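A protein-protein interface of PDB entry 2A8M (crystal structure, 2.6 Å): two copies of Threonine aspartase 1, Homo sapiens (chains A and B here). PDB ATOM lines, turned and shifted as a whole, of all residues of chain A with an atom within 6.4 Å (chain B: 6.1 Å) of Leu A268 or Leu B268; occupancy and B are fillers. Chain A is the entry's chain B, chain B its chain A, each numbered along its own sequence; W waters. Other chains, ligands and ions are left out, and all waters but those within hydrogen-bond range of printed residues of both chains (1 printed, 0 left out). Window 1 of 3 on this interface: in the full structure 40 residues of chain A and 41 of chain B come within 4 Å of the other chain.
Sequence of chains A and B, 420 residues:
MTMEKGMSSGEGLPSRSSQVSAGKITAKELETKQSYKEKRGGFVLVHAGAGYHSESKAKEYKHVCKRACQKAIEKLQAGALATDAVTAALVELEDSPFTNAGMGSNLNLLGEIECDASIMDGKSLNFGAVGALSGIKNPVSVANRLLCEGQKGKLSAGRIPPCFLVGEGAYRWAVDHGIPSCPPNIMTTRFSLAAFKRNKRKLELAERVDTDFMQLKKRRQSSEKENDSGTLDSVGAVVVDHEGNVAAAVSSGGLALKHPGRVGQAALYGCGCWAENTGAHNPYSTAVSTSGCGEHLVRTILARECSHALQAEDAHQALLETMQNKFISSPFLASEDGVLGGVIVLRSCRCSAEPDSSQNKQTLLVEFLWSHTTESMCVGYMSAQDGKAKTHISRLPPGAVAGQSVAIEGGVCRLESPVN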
ATOM      1  N   ASP A 116      22.684  21.774  13.673  1.00  0.00           N
ATOM      2  CA  ASP A 116      23.707  22.709  14.120  1.00  0.00           C
ATOM      3  C   ASP A 116      24.814  22.610  13.059  1.00  0.00           C
ATOM      4  O   ASP A 116      24.945  21.584  12.387  1.00  0.00           O
ATOM      5  CB  ASP A 116      24.266  22.326  15.493  1.00  0.00           C
ATOM      6  CG  ASP A 116      23.179  22.039  16.534  1.00  0.00           C
ATOM      7  OD1 ASP A 116      22.197  22.813  16.648  1.00  0.00           O
ATOM      8  OD2 ASP A 116      23.325  21.032  17.262  1.00  0.00           O
ATOM      9  N   ALA A 117      25.589  23.673  12.878  1.00  0.00           N
ATOM     10  CA  ALA A 117      26.670  23.655  11.894  1.00  0.00           C
ATOM     11  C   ALA A 117      27.482  24.924  11.986  1.00  0.00           C
ATOM     12  O   ALA A 117      26.966  25.981  12.333  1.00  0.00           O
ATOM     13  CB  ALA A 117      26.114  23.495  10.492  1.00  0.00           C
ATOM     14  N   SER A 118      28.765  24.815  11.678  1.00  0.00           N
ATOM     15  CA  SER A 118      29.647  25.970  11.748  1.00  0.00           C
ATOM     16  C   SER A 118      30.801  25.835  10.765  1.00  0.00           C
ATOM     17  O   SER A 118      31.009  24.766  10.190  1.00  0.00           O
ATOM     18  CB  SER A 118      30.172  26.128  13.177  1.00  0.00           C
ATOM     19  OG  SER A 118      30.681  24.904  13.674  1.00  0.00           O
ATOM     20  N   PHE A 127      34.085  33.186  11.617  1.00  0.00           N
ATOM     21  CA  PHE A 127      33.323  32.005  12.010  1.00  0.00           C
ATOM     22  C   PHE A 127      31.852  32.200  11.663  1.00  0.00           C
ATOM     23  O   PHE A 127      31.323  33.313  11.703  1.00  0.00           O
ATOM     24  CB  PHE A 127      33.494  31.816  13.518  1.00  0.00           C
ATOM     25  CG  PHE A 127      32.871  30.576  14.071  1.00  0.00           C
ATOM     26  CD1 PHE A 127      33.434  29.322  13.828  1.00  0.00           C
ATOM     27  CD2 PHE A 127      31.755  30.659  14.905  1.00  0.00           C
ATOM     28  CE1 PHE A 127      32.901  28.169  14.415  1.00  0.00           C
ATOM     29  CE2 PHE A 127      31.214  29.513  15.497  1.00  0.00           C
ATOM     30  CZ  PHE A 127      31.786  28.267  15.255  1.00  0.00           C
ATOM     31  N   ALA A 129      28.046  30.188  12.370  1.00  0.00           N
ATOM     32  CA  ALA A 129      27.320  29.085  12.999  1.00  0.00           C
ATOM     33  C   ALA A 129      25.813  29.265  13.091  1.00  0.00           C
ATOM     34  O   ALA A 129      25.311  30.382  13.244  1.00  0.00           O
ATOM     35  CB  ALA A 129      27.871  28.841  14.404  1.00  0.00           C
ATOM     36  N   PHE A 164      26.634  33.950  14.904  1.00  0.00           N
ATOM     37  CA  PHE A 164      25.871  32.846  15.475  1.00  0.00           C
ATOM     38  C   PHE A 164      24.378  33.136  15.584  1.00  0.00           C
ATOM     39  O   PHE A 164      23.963  33.996  16.357  1.00  0.00           O
ATOM     40  CB  PHE A 164      26.429  32.507  16.856  1.00  0.00           C
ATOM     41  CG  PHE A 164      25.789  31.308  17.503  1.00  0.00           C
ATOM     42  CD1 PHE A 164      25.385  30.216  16.745  1.00  0.00           C
ATOM     43  CD2 PHE A 164      25.680  31.231  18.888  1.00  0.00           C
ATOM     44  CE1 PHE A 164      24.884  29.057  17.356  1.00  0.00           C
ATOM     45  CE2 PHE A 164      25.185  30.082  19.501  1.00  0.00           C
ATOM     46  CZ  PHE A 164      24.789  28.997  18.727  1.00  0.00           C
ATOM     47  N   VAL A 263      21.213  22.588  21.601  1.00  0.00           N
ATOM     48  CA  VAL A 263      22.358  22.854  20.748  1.00  0.00           C
ATOM     49  C   VAL A 263      23.593  22.063  21.157  1.00  0.00           C
ATOM     50  O   VAL A 263      23.883  21.915  22.328  1.00  0.00           O
ATOM     51  CB  VAL A 263      22.695  24.354  20.765  1.00  0.00           C
ATOM     52  CG1 VAL A 263      23.841  24.657  19.800  1.00  0.00           C
ATOM     53  CG2 VAL A 263      21.448  25.167  20.399  1.00  0.00           C
ATOM     54  N   GLY A 264      24.317  21.553  20.171  1.00  0.00           N
ATOM     55  CA  GLY A 264      25.522  20.784  20.446  1.00  0.00           C
ATOM     56  C   GLY A 264      26.786  21.424  19.886  1.00  0.00           C
ATOM     57  O   GLY A 264      26.770  22.575  19.446  1.00  0.00           O
ATOM     58  N   GLN A 265      27.882  20.667  19.914  1.00  0.00           N
ATOM     59  CA  GLN A 265      29.198  21.106  19.427  1.00  0.00           C
ATOM     60  C   GLN A 265      29.218  21.691  18.008  1.00  0.00           C
ATOM     61  O   GLN A 265      29.800  22.750  17.776  1.00  0.00           O
ATOM     62  CB  GLN A 265      30.174  19.926  19.509  1.00  0.00           C
ATOM     63  CG  GLN A 265      29.515  18.597  19.127  1.00  0.00           C
ATOM     64  CD  GLN A 265      29.761  18.188  17.689  1.00  0.00           C
ATOM     65  OE1 GLN A 265      29.037  17.360  17.126  1.00  0.00           O
ATOM     66  NE2 GLN A 265      30.808  18.740  17.097  1.00  0.00           N
ATOM     67  N   ALA A 266      28.582  21.006  17.063  1.00  0.00           N
ATOM     68  CA  ALA A 266      28.558  21.463  15.672  1.00  0.00           C
ATOM     69  C   ALA A 266      28.241  22.943  15.489  1.00  0.00           C
ATOM     70  O   ALA A 266      28.493  23.508  14.425  1.00  0.00           O
ATOM     71  CB  ALA A 266      27.567  20.634  14.863  1.00  0.00           C
ATOM     72  N   ALA A 267      27.699  23.575  16.519  1.00  0.00           N
ATOM     73  CA  ALA A 267      27.341  24.979  16.412  1.00  0.00           C
ATOM     74  C   ALA A 267      28.141  25.903  17.325  1.00  0.00           C
ATOM     75  O   ALA A 267      28.043  27.115  17.196  1.00  0.00           O
ATOM     76  CB  ALA A 267      25.846  25.142  16.691  1.00  0.00           C
ATOM     77  N   LEU A 268      28.938  25.335  18.226  1.00  0.00           N
ATOM     78  CA  LEU A 268      29.700  26.141  19.172  1.00  0.00           C
ATOM     79  C   LEU A 268      31.160  26.396  18.870  1.00  0.00           C
ATOM     80  O   LEU A 268      31.972  25.471  18.745  1.00  0.00           O
ATOM     81  CB  LEU A 268      29.599  25.559  20.578  1.00  0.00           C
ATOM     82  CG  LEU A 268      28.207  25.517  21.189  1.00  0.00           C
ATOM     83  CD1 LEU A 268      28.349  25.196  22.663  1.00  0.00           C
ATOM     84  CD2 LEU A 268      27.495  26.851  21.005  1.00  0.00           C
ATOM     85  N   TYR A 269      31.472  27.685  18.784  1.00  0.00           N
ATOM     86  CA  TYR A 269      32.811  28.173  18.512  1.00  0.00           C
ATOM     87  C   TYR A 269      33.848  27.401  19.339  1.00  0.00           C
ATOM     88  O   TYR A 269      33.631  27.132  20.520  1.00  0.00           O
ATOM     89  CB  TYR A 269      32.851  29.661  18.846  1.00  0.00           C
ATOM     90  CG  TYR A 269      34.151  30.346  18.568  1.00  0.00           C
ATOM     91  CD1 TYR A 269      34.568  30.591  17.265  1.00  0.00           C
ATOM     92  CD2 TYR A 269      34.980  30.736  19.611  1.00  0.00           C
ATOM     93  CE1 TYR A 269      35.784  31.203  17.012  1.00  0.00           C
ATOM     94  CE2 TYR A 269      36.197  31.348  19.370  1.00  0.00           C
ATOM     95  CZ  TYR A 269      36.595  31.575  18.071  1.00  0.00           C
ATOM     96  OH  TYR A 269      37.822  32.147  17.841  1.00  0.00           O
ATOM     97  N   GLY A 270      34.954  27.026  18.696  1.00  0.00           N
ATOM     98  CA  GLY A 270      36.023  26.309  19.372  1.00  0.00           C
ATOM     99  C   GLY A 270      35.726  24.889  19.813  1.00  0.00           C
ATOM    100  O   GLY A 270      36.590  24.223  20.379  1.00  0.00           O
ATOM    101  N   CYS A 271      34.511  24.413  19.563  1.00  0.00           N
ATOM    102  CA  CYS A 271      34.131  23.058  19.970  1.00  0.00           C
ATOM    103  C   CYS A 271      33.967  22.095  18.799  1.00  0.00           C
ATOM    104  O   CYS A 271      34.600  21.046  18.768  1.00  0.00           O
ATOM    105  CB  CYS A 271      32.829  23.094  20.777  1.00  0.00           C
ATOM    106  SG  CYS A 271      32.917  24.091  22.274  1.00  0.00           S
ATOM    107  N   GLY A 272      33.119  22.464  17.843  1.00  0.00           N
ATOM    108  CA  GLY A 272      32.865  21.613  16.696  1.00  0.00           C
ATOM    109  C   GLY A 272      33.921  21.639  15.605  1.00  0.00           C
ATOM    110  O   GLY A 272      34.162  20.618  14.959  1.00  0.00           O
ATOM    111  N   CYS A 273      34.543  22.794  15.384  1.00  0.00           N
ATOM    112  CA  CYS A 273      35.574  22.910  14.361  1.00  0.00           C
ATOM    113  C   CYS A 273      36.523  24.055  14.660  1.00  0.00           C
ATOM    114  O   CYS A 273      36.234  24.916  15.489  1.00  0.00           O
ATOM    115  CB  CYS A 273      34.943  23.115  12.976  1.00  0.00           C
ATOM    116  SG  CYS A 273      34.200  24.737  12.689  1.00  0.00           S
ATOM    117  N   VAL A 298      31.865  19.722  23.690  1.00  0.00           N
ATOM    118  CA  VAL A 298      31.685  21.099  24.112  1.00  0.00           C
ATOM    119  C   VAL A 298      32.425  21.434  25.404  1.00  0.00           C
ATOM    120  O   VAL A 298      33.162  22.409  25.446  1.00  0.00           O
ATOM    121  CB  VAL A 298      30.179  21.454  24.274  1.00  0.00           C
ATOM    122  CG1 VAL A 298      30.022  22.857  24.843  1.00  0.00           C
ATOM    123  CG2 VAL A 298      29.489  21.387  22.930  1.00  0.00           C
ATOM    124  N   ALA A 303      37.892  20.897  19.808  1.00  0.00           N
ATOM    125  CA  ALA A 303      38.365  21.414  18.529  1.00  0.00           C
ATOM    126  C   ALA A 303      39.515  22.391  18.678  1.00  0.00           C
ATOM    127  O   ALA A 303      40.577  22.201  18.066  1.00  0.00           O
ATOM    128  CB  ALA A 303      37.242  22.066  17.777  1.00  0.00           C
ATOM    129  N   SER B 118      24.179  31.943  31.284  1.00  0.00           N
ATOM    130  CA  SER B 118      24.882  30.707  31.562  1.00  0.00           C
ATOM    131  C   SER B 118      25.445  30.783  32.970  1.00  0.00           C
ATOM    132  O   SER B 118      25.602  31.881  33.546  1.00  0.00           O
ATOM    133  CB  SER B 118      26.025  30.492  30.573  1.00  0.00           C
ATOM    134  OG  SER B 118      27.012  31.499  30.722  1.00  0.00           O
ATOM    135  N   PHE B 127      27.857  23.007  33.636  1.00  0.00           N
ATOM    136  CA  PHE B 127      27.530  24.260  33.013  1.00  0.00           C
ATOM    137  C   PHE B 127      26.096  24.278  32.509  1.00  0.00           C
ATOM    138  O   PHE B 127      25.627  23.299  31.936  1.00  0.00           O
ATOM    139  CB  PHE B 127      28.514  24.443  31.856  1.00  0.00           C
ATOM    140  CG  PHE B 127      28.249  25.630  30.998  1.00  0.00           C
ATOM    141  CD1 PHE B 127      28.666  26.892  31.391  1.00  0.00           C
ATOM    142  CD2 PHE B 127      27.626  25.477  29.760  1.00  0.00           C
ATOM    143  CE1 PHE B 127      28.471  28.001  30.564  1.00  0.00           C
ATOM    144  CE2 PHE B 127      27.423  26.571  28.924  1.00  0.00           C
ATOM    145  CZ  PHE B 127      27.851  27.841  29.327  1.00  0.00           C
ATOM    146  N   ALA B 129      23.241  26.850  30.335  1.00  0.00           N
ATOM    147  CA  ALA B 129      23.128  28.049  29.510  1.00  0.00           C
ATOM    148  C   ALA B 129      21.902  28.063  28.623  1.00  0.00           C
ATOM    149  O   ALA B 129      21.501  27.035  28.086  1.00  0.00           O
ATOM    150  CB  ALA B 129      24.382  28.203  28.624  1.00  0.00           C
ATOM    151  N   PHE B 164      22.768  23.201  27.238  1.00  0.00           N
ATOM    152  CA  PHE B 164      22.459  24.438  26.531  1.00  0.00           C
ATOM    153  C   PHE B 164      21.225  24.309  25.634  1.00  0.00           C
ATOM    154  O   PHE B 164      21.188  23.459  24.750  1.00  0.00           O
ATOM    155  CB  PHE B 164      23.702  24.846  25.719  1.00  0.00           C
ATOM    156  CG  PHE B 164      23.515  26.047  24.841  1.00  0.00           C
ATOM    157  CD1 PHE B 164      22.872  27.190  25.309  1.00  0.00           C
ATOM    158  CD2 PHE B 164      24.044  26.060  23.557  1.00  0.00           C
ATOM    159  CE1 PHE B 164      22.761  28.337  24.503  1.00  0.00           C
ATOM    160  CE2 PHE B 164      23.944  27.198  22.741  1.00  0.00           C
ATOM    161  CZ  PHE B 164      23.300  28.337  23.218  1.00  0.00           C
ATOM    162  N   VAL B 263      22.578  34.972  19.257  1.00  0.00           N
ATOM    163  CA  VAL B 263      23.060  34.618  20.591  1.00  0.00           C
ATOM    164  C   VAL B 263      24.453  35.185  20.846  1.00  0.00           C
ATOM    165  O   VAL B 263      25.334  35.064  20.002  1.00  0.00           O
ATOM    166  CB  VAL B 263      23.142  33.089  20.762  1.00  0.00           C
ATOM    167  CG1 VAL B 263      23.555  32.750  22.177  1.00  0.00           C
ATOM    168  CG2 VAL B 263      21.815  32.455  20.409  1.00  0.00           C
ATOM    169  N   GLY B 264      24.653  35.776  22.018  1.00  0.00           N
ATOM    170  CA  GLY B 264      25.947  36.345  22.354  1.00  0.00           C
ATOM    171  C   GLY B 264      26.800  35.529  23.319  1.00  0.00           C
ATOM    172  O   GLY B 264      26.571  34.333  23.535  1.00  0.00           O
ATOM    173  N   GLN B 265      27.776  36.190  23.933  1.00  0.00           N
ATOM    174  CA  GLN B 265      28.687  35.511  24.839  1.00  0.00           C
ATOM    175  C   GLN B 265      28.128  34.998  26.165  1.00  0.00           C
ATOM    176  O   GLN B 265      28.710  34.094  26.763  1.00  0.00           O
ATOM    177  CB  GLN B 265      29.914  36.395  25.097  1.00  0.00           C
ATOM    178  CG  GLN B 265      29.999  37.059  26.459  1.00  0.00           C
ATOM    179  CD  GLN B 265      28.997  38.166  26.638  1.00  0.00           C
ATOM    180  OE1 GLN B 265      28.238  38.485  25.722  1.00  0.00           O
ATOM    181  NE2 GLN B 265      28.986  38.765  27.820  1.00  0.00           N
ATOM    182  N   ALA B 266      27.009  35.545  26.628  1.00  0.00           N
ATOM    183  CA  ALA B 266      26.450  35.094  27.899  1.00  0.00           C
ATOM    184  C   ALA B 266      25.851  33.678  27.834  1.00  0.00           C
ATOM    185  O   ALA B 266      25.576  33.058  28.867  1.00  0.00           O
ATOM    186  CB  ALA B 266      25.414  36.081  28.383  1.00  0.00           C
ATOM    187  N   ALA B 267      25.649  33.172  26.620  1.00  0.00           N
ATOM    188  CA  ALA B 267      25.112  31.831  26.438  1.00  0.00           C
ATOM    189  C   ALA B 267      26.225  30.844  26.063  1.00  0.00           C
ATOM    190  O   ALA B 267      26.124  29.651  26.326  1.00  0.00           O
ATOM    191  CB  ALA B 267      24.022  31.838  25.355  1.00  0.00           C
ATOM    192  N   LEU B 268      27.293  31.349  25.460  1.00  0.00           N
ATOM    193  CA  LEU B 268      28.396  30.494  25.036  1.00  0.00           C
ATOM    194  C   LEU B 268      29.403  30.041  26.081  1.00  0.00           C
ATOM    195  O   LEU B 268      30.112  30.842  26.691  1.00  0.00           O
ATOM    196  CB  LEU B 268      29.163  31.151  23.907  1.00  0.00           C
ATOM    197  CG  LEU B 268      28.354  31.426  22.654  1.00  0.00           C
ATOM    198  CD1 LEU B 268      29.321  31.477  21.470  1.00  0.00           C
ATOM    199  CD2 LEU B 268      27.303  30.344  22.463  1.00  0.00           C
ATOM    200  N   TYR B 269      29.466  28.730  26.245  1.00  0.00           N
ATOM    201  CA  TYR B 269      30.381  28.086  27.163  1.00  0.00           C
ATOM    202  C   TYR B 269      31.820  28.615  27.022  1.00  0.00           C
ATOM    203  O   TYR B 269      32.356  28.709  25.912  1.00  0.00           O
ATOM    204  CB  TYR B 269      30.365  26.585  26.888  1.00  0.00           C
ATOM    205  CG  TYR B 269      31.279  25.773  27.772  1.00  0.00           C
ATOM    206  CD1 TYR B 269      30.974  25.573  29.115  1.00  0.00           C
ATOM    207  CD2 TYR B 269      32.425  25.163  27.255  1.00  0.00           C
ATOM    208  CE1 TYR B 269      31.774  24.782  29.913  1.00  0.00           C
ATOM    209  CE2 TYR B 269      33.229  24.371  28.048  1.00  0.00           C
ATOM    210  CZ  TYR B 269      32.895  24.181  29.373  1.00  0.00           C
ATOM    211  OH  TYR B 269      33.649  23.358  30.167  1.00  0.00           O
ATOM    212  N   GLY B 270      32.439  28.941  28.152  1.00  0.00           N
ATOM    213  CA  GLY B 270      33.808  29.435  28.145  1.00  0.00           C
ATOM    214  C   GLY B 270      33.963  30.903  27.797  1.00  0.00           C
ATOM    215  O   GLY B 270      35.051  31.467  27.925  1.00  0.00           O
ATOM    216  N   CYS B 271      32.876  31.533  27.367  1.00  0.00           N
ATOM    217  CA  CYS B 271      32.916  32.940  26.984  1.00  0.00           C
ATOM    218  C   CYS B 271      32.333  33.860  28.058  1.00  0.00           C
ATOM    219  O   CYS B 271      33.049  34.690  28.620  1.00  0.00           O
ATOM    220  CB  CYS B 271      32.187  33.129  25.644  1.00  0.00           C
ATOM    221  SG  CYS B 271      32.847  32.093  24.278  1.00  0.00           S
ATOM    222  N   GLY B 272      31.044  33.707  28.347  1.00  0.00           N
ATOM    223  CA  GLY B 272      30.411  34.532  29.358  1.00  0.00           C
ATOM    224  C   GLY B 272      30.984  34.335  30.750  1.00  0.00           C
ATOM    225  O   GLY B 272      31.328  35.311  31.431  1.00  0.00           O
ATOM    226  N   CYS B 273      31.088  33.083  31.185  1.00  0.00           N
ATOM    227  CA  CYS B 273      31.626  32.787  32.511  1.00  0.00           C
ATOM    228  C   CYS B 273      32.450  31.511  32.553  1.00  0.00           C
ATOM    229  O   CYS B 273      32.442  30.706  31.629  1.00  0.00           O
ATOM    230  CB  CYS B 273      30.494  32.667  33.532  1.00  0.00           C
ATOM    231  SG  CYS B 273      29.307  31.347  33.174  1.00  0.00           S
ATOM    232  N   VAL B 298      33.611  36.266  22.533  1.00  0.00           N
ATOM    233  CA  VAL B 298      33.496  34.913  22.014  1.00  0.00           C
ATOM    234  C   VAL B 298      34.678  34.557  21.141  1.00  0.00           C
ATOM    235  O   VAL B 298      35.334  33.544  21.370  1.00  0.00           O
ATOM    236  CB  VAL B 298      32.194  34.719  21.202  1.00  0.00           C
ATOM    237  CG1 VAL B 298      32.130  33.316  20.647  1.00  0.00           C
ATOM    238  CG2 VAL B 298      30.992  34.996  22.090  1.00  0.00           C
HETATM  239  O   HOH W   1      23.344  20.863  24.944  1.00  0.00           O
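Among the printed residues, merely in contact across the chains: Phe A164 with Leu B268, Leu A268 with Phe B164, Leu A268 with Leu B268, Tyr A269 with Val B298 and Val A298 with Tyr B269.
O of Tyr B269 is in hydrogen-bond range of SG of Cys B271 (3.8 Å).
O of Tyr A269 is in hydrogen-bond range of SG of Cys A271 (3.6 Å).
O of Val A298 is in hydrogen-bond range of SG of Cys A271 (3.6 Å).
Leu B268 touches two residues of chain A.
Printed residues of chain A within 4 Å of Phe B164: Val A263 and Leu A268.
Of the printed residues of chain B, Val A263 touches Phe B164.
Printed residues of chain B within 4 Å of Tyr A269: Val B298 (3.1 Å).
Of the printed residues of chain A, Val B263 touches Phe A164.
Ala B129 touches none of the printed residues of chain A.
The nearest residue of chain B that does not touch Leu A268 is Tyr B269 (4.9 Å).
Water W1 lies within hydrogen-bond range of the backbone carbonyl oxygen (O) of Val A263 (2.9 Å) and the backbone NH (N) of Phe B164 (3.3 Å).
Phe A164 touches Val B263, and with the chains exchanged Val A263 touches Phe B164.
Phe A164 touches Leu B268, and with the chains exchanged Leu A268 touches Phe B164.
Leu A268 touches its own counterpart, Leu B268.
Tyr A269 touches Val B298, and with the chains exchanged Val A298 touches Tyr B269.
Positions printed for both chains: 118, 127, 129, 164, 263, 264, 265, 266, 267, 268, 269, 270, 271, 272, 273 and 298.
Hydrophobic or aromatic side chains of chain A within 4 Å of the printed part of chain B: Phe A164, Val A263, Leu A268 and Tyr A269.
Among the printed residues, 7 pairs touch across the chains.
The backbone carbonyl oxygen (O) of Phe B164 lies within hydrogen-bond range of the backbone NH (N) of Val A263 (3.3 Å).
The backbone carbonyl oxygen of Phe A164 sits at hydrogen-bond distance from the backbone NH of Val B263, at 3.4 Å.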
